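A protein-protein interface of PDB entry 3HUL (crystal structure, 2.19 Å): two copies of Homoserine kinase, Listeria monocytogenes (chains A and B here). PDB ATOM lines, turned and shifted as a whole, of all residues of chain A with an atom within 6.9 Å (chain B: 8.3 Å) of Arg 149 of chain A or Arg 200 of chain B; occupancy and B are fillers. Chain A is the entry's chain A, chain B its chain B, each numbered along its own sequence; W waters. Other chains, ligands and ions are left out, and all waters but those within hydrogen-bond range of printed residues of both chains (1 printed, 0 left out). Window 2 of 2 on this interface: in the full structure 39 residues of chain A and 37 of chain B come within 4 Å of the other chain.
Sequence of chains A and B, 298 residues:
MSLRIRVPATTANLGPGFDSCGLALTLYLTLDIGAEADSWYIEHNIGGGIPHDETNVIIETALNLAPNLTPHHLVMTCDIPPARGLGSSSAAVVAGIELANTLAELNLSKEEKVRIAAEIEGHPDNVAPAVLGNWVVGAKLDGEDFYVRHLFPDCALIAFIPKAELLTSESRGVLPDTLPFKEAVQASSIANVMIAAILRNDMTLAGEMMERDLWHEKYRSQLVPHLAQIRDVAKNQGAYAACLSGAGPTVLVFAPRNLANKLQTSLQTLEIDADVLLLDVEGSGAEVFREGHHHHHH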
ATOM      1  N   LEU A 132       7.673 -13.198  33.458  1.00  0.00           N
ATOM      2  CA  LEU A 132       6.830 -14.321  33.919  1.00  0.00           C
ATOM      3  C   LEU A 132       7.467 -15.086  35.052  1.00  0.00           C
ATOM      4  O   LEU A 132       6.784 -15.737  35.839  1.00  0.00           O
ATOM      5  CB  LEU A 132       6.554 -15.249  32.763  1.00  0.00           C
ATOM      6  CG  LEU A 132       5.878 -14.497  31.609  1.00  0.00           C
ATOM      7  CD1 LEU A 132       5.721 -15.448  30.474  1.00  0.00           C
ATOM      8  CD2 LEU A 132       4.511 -13.894  32.060  1.00  0.00           C
ATOM      9  N   GLY A 133       8.787 -14.971  35.143  1.00  0.00           N
ATOM     10  CA  GLY A 133       9.538 -15.653  36.169  1.00  0.00           C
ATOM     11  C   GLY A 133       9.847 -17.071  35.709  1.00  0.00           C
ATOM     12  O   GLY A 133       9.250 -17.590  34.768  1.00  0.00           O
ATOM     13  N   ASN A 134      10.800 -17.677  36.397  1.00  0.00           N
ATOM     14  CA  ASN A 134      11.164 -19.055  36.186  1.00  0.00           C
ATOM     15  C   ASN A 134      11.684 -19.348  34.774  1.00  0.00           C
ATOM     16  O   ASN A 134      12.442 -18.563  34.212  1.00  0.00           O
ATOM     17  CB  ASN A 134       9.986 -19.964  36.584  1.00  0.00           C
ATOM     18  CG  ASN A 134      10.436 -21.125  37.406  1.00  0.00           C
ATOM     19  OD1 ASN A 134      11.373 -21.834  37.024  1.00  0.00           O
ATOM     20  ND2 ASN A 134       9.799 -21.322  38.553  1.00  0.00           N
ATOM     21  N   TRP A 135      11.254 -20.466  34.205  1.00  0.00           N
ATOM     22  CA  TRP A 135      11.784 -20.958  32.922  1.00  0.00           C
ATOM     23  C   TRP A 135      10.683 -20.804  31.878  1.00  0.00           C
ATOM     24  O   TRP A 135       9.545 -21.269  32.090  1.00  0.00           O
ATOM     25  CB  TRP A 135      12.289 -22.405  33.068  1.00  0.00           C
ATOM     26  CG  TRP A 135      12.581 -23.122  31.781  1.00  0.00           C
ATOM     27  CD1 TRP A 135      13.215 -22.622  30.679  1.00  0.00           C
ATOM     28  CD2 TRP A 135      12.244 -24.477  31.466  1.00  0.00           C
ATOM     29  NE1 TRP A 135      13.286 -23.575  29.699  1.00  0.00           N
ATOM     30  CE2 TRP A 135      12.693 -24.724  30.151  1.00  0.00           C
ATOM     31  CE3 TRP A 135      11.637 -25.516  32.183  1.00  0.00           C
ATOM     32  CZ2 TRP A 135      12.554 -25.978  29.524  1.00  0.00           C
ATOM     33  CZ3 TRP A 135      11.467 -26.756  31.557  1.00  0.00           C
ATOM     34  CH2 TRP A 135      11.920 -26.970  30.228  1.00  0.00           C
ATOM     35  N   VAL A 136      11.002 -20.095  30.794  1.00  0.00           N
ATOM     36  CA  VAL A 136      10.041 -19.894  29.698  1.00  0.00           C
ATOM     37  C   VAL A 136      10.569 -20.476  28.404  1.00  0.00           C
ATOM     38  O   VAL A 136      11.717 -20.222  28.035  1.00  0.00           O
ATOM     39  CB  VAL A 136       9.678 -18.407  29.478  1.00  0.00           C
ATOM     40  CG1 VAL A 136       8.490 -18.264  28.407  1.00  0.00           C
ATOM     41  CG2 VAL A 136       9.273 -17.797  30.786  1.00  0.00           C
ATOM     42  N   VAL A 137       9.743 -21.298  27.760  1.00  0.00           N
ATOM     43  CA  VAL A 137      10.003 -21.758  26.400  1.00  0.00           C
ATOM     44  C   VAL A 137       9.125 -20.914  25.481  1.00  0.00           C
ATOM     45  O   VAL A 137       7.896 -20.868  25.641  1.00  0.00           O
ATOM     46  CB  VAL A 137       9.677 -23.260  26.215  1.00  0.00           C
ATOM     47  CG1 VAL A 137       9.828 -23.704  24.734  1.00  0.00           C
ATOM     48  CG2 VAL A 137      10.507 -24.111  27.134  1.00  0.00           C
ATOM     49  N   TYR A 147       4.390 -18.830  24.250  1.00  0.00           N
ATOM     50  CA  TYR A 147       5.303 -19.163  25.322  1.00  0.00           C
ATOM     51  C   TYR A 147       4.628 -20.103  26.313  1.00  0.00           C
ATOM     52  O   TYR A 147       3.401 -20.112  26.437  1.00  0.00           O
ATOM     53  CB  TYR A 147       5.866 -17.887  26.002  1.00  0.00           C
ATOM     54  CG  TYR A 147       4.845 -17.000  26.662  1.00  0.00           C
ATOM     55  CD1 TYR A 147       4.254 -17.379  27.866  1.00  0.00           C
ATOM     56  CD2 TYR A 147       4.462 -15.767  26.089  1.00  0.00           C
ATOM     57  CE1 TYR A 147       3.296 -16.573  28.507  1.00  0.00           C
ATOM     58  CE2 TYR A 147       3.495 -14.942  26.719  1.00  0.00           C
ATOM     59  CZ  TYR A 147       2.928 -15.361  27.937  1.00  0.00           C
ATOM     60  OH  TYR A 147       1.984 -14.609  28.612  1.00  0.00           O
ATOM     61  N   VAL A 148       5.437 -20.938  26.952  1.00  0.00           N
ATOM     62  CA  VAL A 148       4.974 -21.774  28.044  1.00  0.00           C
ATOM     63  C   VAL A 148       5.943 -21.560  29.184  1.00  0.00           C
ATOM     64  O   VAL A 148       7.163 -21.625  28.975  1.00  0.00           O
ATOM     65  CB  VAL A 148       4.945 -23.292  27.670  1.00  0.00           C
ATOM     66  CG1 VAL A 148       4.362 -24.103  28.818  1.00  0.00           C
ATOM     67  CG2 VAL A 148       4.115 -23.543  26.413  1.00  0.00           C
ATOM     68  N   ARG A 149       5.403 -21.296  30.367  1.00  0.00           N
ATOM     69  CA  ARG A 149       6.204 -21.233  31.588  1.00  0.00           C
ATOM     70  C   ARG A 149       6.184 -22.572  32.326  1.00  0.00           C
ATOM     71  O   ARG A 149       5.134 -23.113  32.604  1.00  0.00           O
ATOM     72  CB  ARG A 149       5.720 -20.112  32.520  1.00  0.00           C
ATOM     73  CG  ARG A 149       6.387 -20.094  33.923  1.00  0.00           C
ATOM     74  CD  ARG A 149       5.673 -19.015  34.774  1.00  0.00           C
ATOM     75  NE  ARG A 149       6.341 -18.652  36.021  1.00  0.00           N
ATOM     76  CZ  ARG A 149       6.165 -19.257  37.198  1.00  0.00           C
ATOM     77  NH1 ARG A 149       5.352 -20.307  37.303  1.00  0.00           N
ATOM     78  NH2 ARG A 149       6.814 -18.821  38.277  1.00  0.00           N
ATOM     79  N   HIS A 150       7.367 -23.076  32.646  1.00  0.00           N
ATOM     80  CA  HIS A 150       7.526 -24.291  33.401  1.00  0.00           C
ATOM     81  C   HIS A 150       8.389 -23.983  34.637  1.00  0.00           C
ATOM     82  O   HIS A 150       9.028 -22.917  34.714  1.00  0.00           O
ATOM     83  CB  HIS A 150       8.197 -25.372  32.529  1.00  0.00           C
ATOM     84  CG  HIS A 150       7.237 -26.156  31.689  1.00  0.00           C
ATOM     85  ND1 HIS A 150       6.355 -27.075  32.226  1.00  0.00           N
ATOM     86  CD2 HIS A 150       7.019 -26.165  30.350  1.00  0.00           C
ATOM     87  CE1 HIS A 150       5.647 -27.622  31.250  1.00  0.00           C
ATOM     88  NE2 HIS A 150       6.021 -27.084  30.103  1.00  0.00           N
ATOM     89  N   LEU A 151       8.366 -24.885  35.612  1.00  0.00           N
ATOM     90  CA  LEU A 151       9.266 -24.815  36.756  1.00  0.00           C
ATOM     91  C   LEU A 151      10.566 -25.458  36.414  1.00  0.00           C
ATOM     92  O   LEU A 151      10.588 -26.626  36.039  1.00  0.00           O
ATOM     93  CB  LEU A 151       8.760 -25.685  37.869  1.00  0.00           C
ATOM     94  CG  LEU A 151       7.686 -25.203  38.787  1.00  0.00           C
ATOM     95  CD1 LEU A 151       6.312 -25.308  38.081  1.00  0.00           C
ATOM     96  CD2 LEU A 151       7.862 -26.157  39.989  1.00  0.00           C
ATOM     97  N   LEU A 199      11.742 -31.952  32.052  1.00  0.00           N
ATOM     98  CA  LEU A 199      10.432 -32.302  32.614  1.00  0.00           C
ATOM     99  C   LEU A 199      10.338 -33.745  33.177  1.00  0.00           C
ATOM    100  O   LEU A 199       9.360 -34.075  33.854  1.00  0.00           O
ATOM    101  CB  LEU A 199       9.278 -31.891  31.646  1.00  0.00           C
ATOM    102  CG  LEU A 199       9.171 -30.330  31.652  1.00  0.00           C
ATOM    103  CD1 LEU A 199       8.896 -29.705  30.311  1.00  0.00           C
ATOM    104  CD2 LEU A 199       8.090 -29.898  32.650  1.00  0.00           C
ATOM    105  N   GLU A 282      14.861 -17.610  39.819  1.00  0.00           N
ATOM    106  CA  GLU A 282      13.885 -16.684  40.392  1.00  0.00           C
ATOM    107  C   GLU A 282      12.489 -17.009  39.824  1.00  0.00           C
ATOM    108  O   GLU A 282      12.251 -16.920  38.614  1.00  0.00           O
ATOM    109  CB  GLU A 282      14.311 -15.213  40.146  1.00  0.00           C
ATOM    110  CG  GLU A 282      13.258 -14.145  40.485  1.00  0.00           C
ATOM    111  CD  GLU A 282      12.742 -14.248  41.921  1.00  0.00           C
ATOM    112  OE1 GLU A 282      13.516 -13.977  42.866  1.00  0.00           O
ATOM    113  OE2 GLU A 282      11.553 -14.588  42.110  1.00  0.00           O
ATOM    114  N   GLY A 283      11.590 -17.403  40.715  1.00  0.00           N
ATOM    115  CA  GLY A 283      10.256 -17.840  40.358  1.00  0.00           C
ATOM    116  C   GLY A 283       9.302 -16.731  39.969  1.00  0.00           C
ATOM    117  O   GLY A 283       8.358 -16.980  39.228  1.00  0.00           O
ATOM    118  N   SER A 284       9.543 -15.508  40.461  1.00  0.00           N
ATOM    119  CA  SER A 284       8.623 -14.391  40.218  1.00  0.00           C
ATOM    120  C   SER A 284       9.151 -13.504  39.115  1.00  0.00           C
ATOM    121  O   SER A 284      10.331 -13.179  39.085  1.00  0.00           O
ATOM    122  CB  SER A 284       8.477 -13.538  41.473  1.00  0.00           C
ATOM    123  OG  SER A 284       8.230 -14.347  42.610  1.00  0.00           O
ATOM    124  N   GLY A 285       8.282 -13.086  38.213  1.00  0.00           N
ATOM    125  CA  GLY A 285       8.696 -12.127  37.227  1.00  0.00           C
ATOM    126  C   GLY A 285       8.676 -10.720  37.812  1.00  0.00           C
ATOM    127  O   GLY A 285       8.529 -10.533  39.021  1.00  0.00           O
ATOM    128  N   TRP B 135       4.601 -41.539  23.989  1.00  0.00           N
ATOM    129  CA  TRP B 135       5.167 -40.405  23.239  1.00  0.00           C
ATOM    130  C   TRP B 135       6.690 -40.365  23.483  1.00  0.00           C
ATOM    131  O   TRP B 135       7.148 -40.462  24.623  1.00  0.00           O
ATOM    132  CB  TRP B 135       4.492 -39.094  23.707  1.00  0.00           C
ATOM    133  CG  TRP B 135       5.023 -37.828  23.109  1.00  0.00           C
ATOM    134  CD1 TRP B 135       5.406 -37.620  21.807  1.00  0.00           C
ATOM    135  CD2 TRP B 135       5.197 -36.585  23.779  1.00  0.00           C
ATOM    136  NE1 TRP B 135       5.815 -36.328  21.634  1.00  0.00           N
ATOM    137  CE2 TRP B 135       5.700 -35.668  22.835  1.00  0.00           C
ATOM    138  CE3 TRP B 135       4.970 -36.152  25.098  1.00  0.00           C
ATOM    139  CZ2 TRP B 135       6.021 -34.354  23.167  1.00  0.00           C
ATOM    140  CZ3 TRP B 135       5.280 -34.827  25.421  1.00  0.00           C
ATOM    141  CH2 TRP B 135       5.796 -33.949  24.455  1.00  0.00           C
ATOM    142  N   LEU B 151       4.265 -39.409  28.888  1.00  0.00           N
ATOM    143  CA  LEU B 151       2.876 -39.806  28.781  1.00  0.00           C
ATOM    144  C   LEU B 151       2.075 -38.676  28.099  1.00  0.00           C
ATOM    145  O   LEU B 151       1.915 -37.586  28.662  1.00  0.00           O
ATOM    146  CB  LEU B 151       2.301 -40.071  30.181  1.00  0.00           C
ATOM    147  CG  LEU B 151       3.183 -41.033  31.021  1.00  0.00           C
ATOM    148  CD1 LEU B 151       2.614 -41.231  32.418  1.00  0.00           C
ATOM    149  CD2 LEU B 151       3.411 -42.376  30.276  1.00  0.00           C
ATOM    150  N   PRO B 153      -0.905 -36.471  26.976  1.00  0.00           N
ATOM    151  CA  PRO B 153      -2.185 -36.129  27.555  1.00  0.00           C
ATOM    152  C   PRO B 153      -3.327 -36.960  26.948  1.00  0.00           C
ATOM    153  O   PRO B 153      -3.357 -37.224  25.744  1.00  0.00           O
ATOM    154  CB  PRO B 153      -2.368 -34.654  27.166  1.00  0.00           C
ATOM    155  CG  PRO B 153      -0.931 -34.113  27.129  1.00  0.00           C
ATOM    156  CD  PRO B 153      -0.188 -35.286  26.466  1.00  0.00           C
ATOM    157  N   VAL B 193       7.982 -24.957  21.772  1.00  0.00           N
ATOM    158  CA  VAL B 193       6.764 -24.525  22.445  1.00  0.00           C
ATOM    159  C   VAL B 193       5.699 -25.647  22.400  1.00  0.00           C
ATOM    160  O   VAL B 193       5.038 -25.898  23.409  1.00  0.00           O
ATOM    161  CB  VAL B 193       6.215 -23.203  21.819  1.00  0.00           C
ATOM    162  CG1 VAL B 193       4.800 -22.857  22.351  1.00  0.00           C
ATOM    163  CG2 VAL B 193       7.180 -22.054  22.087  1.00  0.00           C
ATOM    164  N   MET B 194       5.554 -26.320  21.246  1.00  0.00           N
ATOM    165  CA  MET B 194       4.640 -27.472  21.122  1.00  0.00           C
ATOM    166  C   MET B 194       4.951 -28.477  22.244  1.00  0.00           C
ATOM    167  O   MET B 194       4.080 -28.885  22.994  1.00  0.00           O
ATOM    168  CB  MET B 194       4.814 -28.167  19.778  1.00  0.00           C
ATOM    169  CG  MET B 194       3.861 -29.370  19.609  1.00  0.00           C
ATOM    170  SD  MET B 194       3.984 -30.238  18.034  1.00  0.00           S
ATOM    171  CE  MET B 194       5.533 -31.062  18.189  1.00  0.00           C
ATOM    172  N   ILE B 195       6.223 -28.819  22.391  1.00  0.00           N
ATOM    173  CA  ILE B 195       6.594 -29.813  23.372  1.00  0.00           C
ATOM    174  C   ILE B 195       6.305 -29.315  24.779  1.00  0.00           C
ATOM    175  O   ILE B 195       5.736 -30.035  25.571  1.00  0.00           O
ATOM    176  CB  ILE B 195       8.035 -30.237  23.165  1.00  0.00           C
ATOM    177  CG1 ILE B 195       8.115 -31.021  21.843  1.00  0.00           C
ATOM    178  CG2 ILE B 195       8.544 -31.067  24.328  1.00  0.00           C
ATOM    179  CD1 ILE B 195       9.512 -31.143  21.289  1.00  0.00           C
ATOM    180  N   ALA B 196       6.656 -28.064  25.077  1.00  0.00           N
ATOM    181  CA  ALA B 196       6.430 -27.535  26.415  1.00  0.00           C
ATOM    182  C   ALA B 196       4.942 -27.523  26.726  1.00  0.00           C
ATOM    183  O   ALA B 196       4.532 -27.706  27.904  1.00  0.00           O
ATOM    184  CB  ALA B 196       7.020 -26.133  26.551  1.00  0.00           C
ATOM    185  N   ALA B 197       4.144 -27.287  25.678  1.00  0.00           N
ATOM    186  CA  ALA B 197       2.696 -27.135  25.825  1.00  0.00           C
ATOM    187  C   ALA B 197       2.074 -28.478  26.116  1.00  0.00           C
ATOM    188  O   ALA B 197       1.260 -28.596  27.047  1.00  0.00           O
ATOM    189  CB  ALA B 197       2.051 -26.447  24.516  1.00  0.00           C
ATOM    190  N   ILE B 198       2.486 -29.505  25.358  1.00  0.00           N
ATOM    191  CA  ILE B 198       1.977 -30.868  25.576  1.00  0.00           C
ATOM    192  C   ILE B 198       2.279 -31.280  27.032  1.00  0.00           C
ATOM    193  O   ILE B 198       1.437 -31.851  27.721  1.00  0.00           O
ATOM    194  CB  ILE B 198       2.622 -31.909  24.585  1.00  0.00           C
ATOM    195  CG1 ILE B 198       2.280 -31.577  23.119  1.00  0.00           C
ATOM    196  CG2 ILE B 198       2.253 -33.345  24.974  1.00  0.00           C
ATOM    197  CD1 ILE B 198       3.081 -32.341  22.090  1.00  0.00           C
ATOM    198  N   LEU B 199       3.485 -30.958  27.482  1.00  0.00           N
ATOM    199  CA  LEU B 199       3.912 -31.329  28.838  1.00  0.00           C
ATOM    200  C   LEU B 199       3.207 -30.559  29.946  1.00  0.00           C
ATOM    201  O   LEU B 199       3.268 -30.984  31.104  1.00  0.00           O
ATOM    202  CB  LEU B 199       5.423 -31.191  28.954  1.00  0.00           C
ATOM    203  CG  LEU B 199       6.193 -32.294  28.204  1.00  0.00           C
ATOM    204  CD1 LEU B 199       7.608 -31.842  27.825  1.00  0.00           C
ATOM    205  CD2 LEU B 199       6.220 -33.562  29.064  1.00  0.00           C
ATOM    206  N   ARG B 200       2.569 -29.426  29.612  1.00  0.00           N
ATOM    207  CA  ARG B 200       1.651 -28.762  30.534  1.00  0.00           C
ATOM    208  C   ARG B 200       0.192 -29.229  30.367  1.00  0.00           C
ATOM    209  O   ARG B 200      -0.703 -28.606  30.938  1.00  0.00           O
ATOM    210  CB  ARG B 200       1.662 -27.236  30.330  1.00  0.00           C
ATOM    211  CG  ARG B 200       2.858 -26.538  30.870  1.00  0.00           C
ATOM    212  CD  ARG B 200       2.519 -25.265  31.666  1.00  0.00           C
ATOM    213  NE  ARG B 200       1.594 -24.335  30.999  1.00  0.00           N
ATOM    214  CZ  ARG B 200       1.227 -23.155  31.510  1.00  0.00           C
ATOM    215  NH1 ARG B 200       0.370 -22.380  30.854  1.00  0.00           N
ATOM    216  NH2 ARG B 200       1.708 -22.741  32.685  1.00  0.00           N
ATOM    217  N   ASN B 201      -0.070 -30.282  29.580  1.00  0.00           N
ATOM    218  CA  ASN B 201      -1.459 -30.705  29.303  1.00  0.00           C
ATOM    219  C   ASN B 201      -2.225 -29.541  28.666  1.00  0.00           C
ATOM    220  O   ASN B 201      -3.424 -29.373  28.889  1.00  0.00           O
ATOM    221  CB  ASN B 201      -2.198 -31.175  30.568  1.00  0.00           C
ATOM    222  CG  ASN B 201      -1.635 -32.470  31.147  1.00  0.00           C
ATOM    223  OD1 ASN B 201      -1.412 -32.573  32.364  1.00  0.00           O
ATOM    224  ND2 ASN B 201      -1.422 -33.476  30.294  1.00  0.00           N
ATOM    225  N   ASP B 202      -1.509 -28.726  27.896  1.00  0.00           N
ATOM    226  CA  ASP B 202      -2.123 -27.610  27.198  1.00  0.00           C
ATOM    227  C   ASP B 202      -2.270 -27.986  25.736  1.00  0.00           C
ATOM    228  O   ASP B 202      -1.479 -27.588  24.864  1.00  0.00           O
ATOM    229  CB  ASP B 202      -1.302 -26.324  27.394  1.00  0.00           C
ATOM    230  CG  ASP B 202      -2.050 -25.086  26.937  1.00  0.00           C
ATOM    231  OD1 ASP B 202      -3.018 -25.208  26.143  1.00  0.00           O
ATOM    232  OD2 ASP B 202      -1.650 -23.986  27.352  1.00  0.00           O
ATOM    233  N   MET B 203      -3.283 -28.788  25.466  1.00  0.00           N
ATOM    234  CA  MET B 203      -3.472 -29.298  24.119  1.00  0.00           C
ATOM    235  C   MET B 203      -3.952 -28.223  23.137  1.00  0.00           C
ATOM    236  O   MET B 203      -3.730 -28.355  21.950  1.00  0.00           O
ATOM    237  CB  MET B 203      -4.363 -30.554  24.124  1.00  0.00           C
ATOM    238  CG  MET B 203      -3.652 -31.854  24.696  1.00  0.00           C
ATOM    239  SD  MET B 203      -2.250 -32.446  23.686  1.00  0.00           S
ATOM    240  CE  MET B 203      -3.117 -32.950  22.188  1.00  0.00           C
ATOM    241  N   LEU B 205      -2.828 -24.922  22.952  1.00  0.00           N
ATOM    242  CA  LEU B 205      -1.589 -24.306  22.470  1.00  0.00           C
ATOM    243  C   LEU B 205      -0.747 -25.309  21.680  1.00  0.00           C
ATOM    244  O   LEU B 205      -0.191 -24.963  20.625  1.00  0.00           O
ATOM    245  CB  LEU B 205      -0.799 -23.713  23.640  1.00  0.00           C
ATOM    246  CG  LEU B 205       0.576 -23.087  23.343  1.00  0.00           C
ATOM    247  CD1 LEU B 205       0.524 -22.054  22.198  1.00  0.00           C
ATOM    248  CD2 LEU B 205       1.095 -22.470  24.644  1.00  0.00           C
ATOM    249  N   ALA B 206      -0.681 -26.561  22.141  1.00  0.00           N
ATOM    250  CA  ALA B 206       0.162 -27.532  21.421  1.00  0.00           C
ATOM    251  C   ALA B 206      -0.356 -27.730  19.998  1.00  0.00           C
ATOM    252  O   ALA B 206       0.423 -27.760  19.023  1.00  0.00           O
ATOM    253  CB  ALA B 206       0.226 -28.889  22.156  1.00  0.00           C
HETATM  254  O   HOH W   1       2.776 -20.486  30.532  1.00  0.00           O
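O of Leu 132 of chain A is in hydrogen-bond range of NE of Arg 149 of chain A, at 3.0 Å. O of Gly 133 of chain A sits at hydrogen-bond distance from NE of Arg 149 of chain A (3.3 Å). The backbone carbonyl oxygen (O) of Trp 135 of chain A sits at hydrogen-bond distance from the backbone NH (N) of His 150 of chain A, at 2.9 Å. The backbone carbonyl oxygen of Val 137 of chain A lies within hydrogen-bond range of the backbone NH of Val 148 of chain A, at 2.8 Å. NH2 of Arg 149 of chain A lies within hydrogen-bond range of O of Gly 283 of chain A (2.6 Å). The backbone NH (N) of Leu 205 of chain B is in hydrogen-bond range of the side-chain carboxylate (OD1) of Asp 202 of chain B (3.2 Å).
Val 137 of chain A touches Val 193 of chain B (CG1 to N, 3.7 Å). Val 137 of chain A touches Ala 196 of chain B. Leu 205 of chain B touches Tyr 147 of chain A (CD2 to O, 3.8 Å). O of Val 193 of chain B touches CG2 of Val 148 of chain A, 3.9 Å away. Ala 196 of chain B touches Val 148 of chain A (CB to CB, 3.7 Å). CG2 of Val 148 of chain A touches N of Ala 197 of chain B, at 3.8 Å. Val 148 of chain A touches Arg 200 of chain B. Val 148 of chain A touches Leu 205 of chain B (CG2 to CD2, 3.7 Å). His 150 of chain A touches Arg 200 of chain B (CE1 to CG, 3.0 Å). CD1 of Leu 199 of chain B touches CD1 of Leu 199 of chain A, at 3.5 Å.
The guanidinium group of Arg 200 of chain B lies within hydrogen-bond range of the backbone carbonyl oxygen of Arg 149 of chain A (3.4 Å). A ring nitrogen (NE2) of His 150 of chain A lies within hydrogen-bond range of the backbone carbonyl oxygen of Ala 196 of chain B, 2.7 Å away.
Hydrophobic or aromatic side chains of chain B within 4 Å of the printed part of chain A: Val 193, Ala 196, Leu 199 and Leu 205. Hydrophobic or aromatic side chains of chain A within 4 Å of the printed part of chain B: Val 137, Val 148, His 150 and Leu 199. Among the printed residues, 12 pairs touch across the chains.
Water W1 lies within hydrogen-bond range of N of Arg 149 of chain A (2.8 Å) and NH1 of Arg 200 of chain B (3.1 Å).
Leu 199 of chain A touches its own counterpart, Leu 199 of chain B. Of the 12 pairs that touch across the chains among the printed residues, 1 has its exchanged pair printed and touching as well.
Leu 132 of chain A touches none of the printed residues of chain B. Of the printed residues of chain B, Val 137 of chain A touches Val 193 (3.7 Å) and Ala 196 (3.9 Å). Of the printed residues of chain B, Tyr 147 of chain A touches Leu 205 (3.8 Å). Of the printed residues of chain B, Arg 149 of chain A touches Arg 200. His 150 of chain A touches two residues of chain B. Gly 283 of chain A touches none of the printed residues of chain B. Of the printed residues of chain A, Val 193 of chain B touches Val 137 and Val 148. Arg 200 of chain B touches just these residues of chain A: Val 148, Arg 149 and His 150. Of the printed residues of chain A, Leu 205 of chain B touches Tyr 147 and Val 148. The nearest printed residue of chain B that does not touch Val 148 of chain A is Asp 202 of chain B (5.9 Å).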
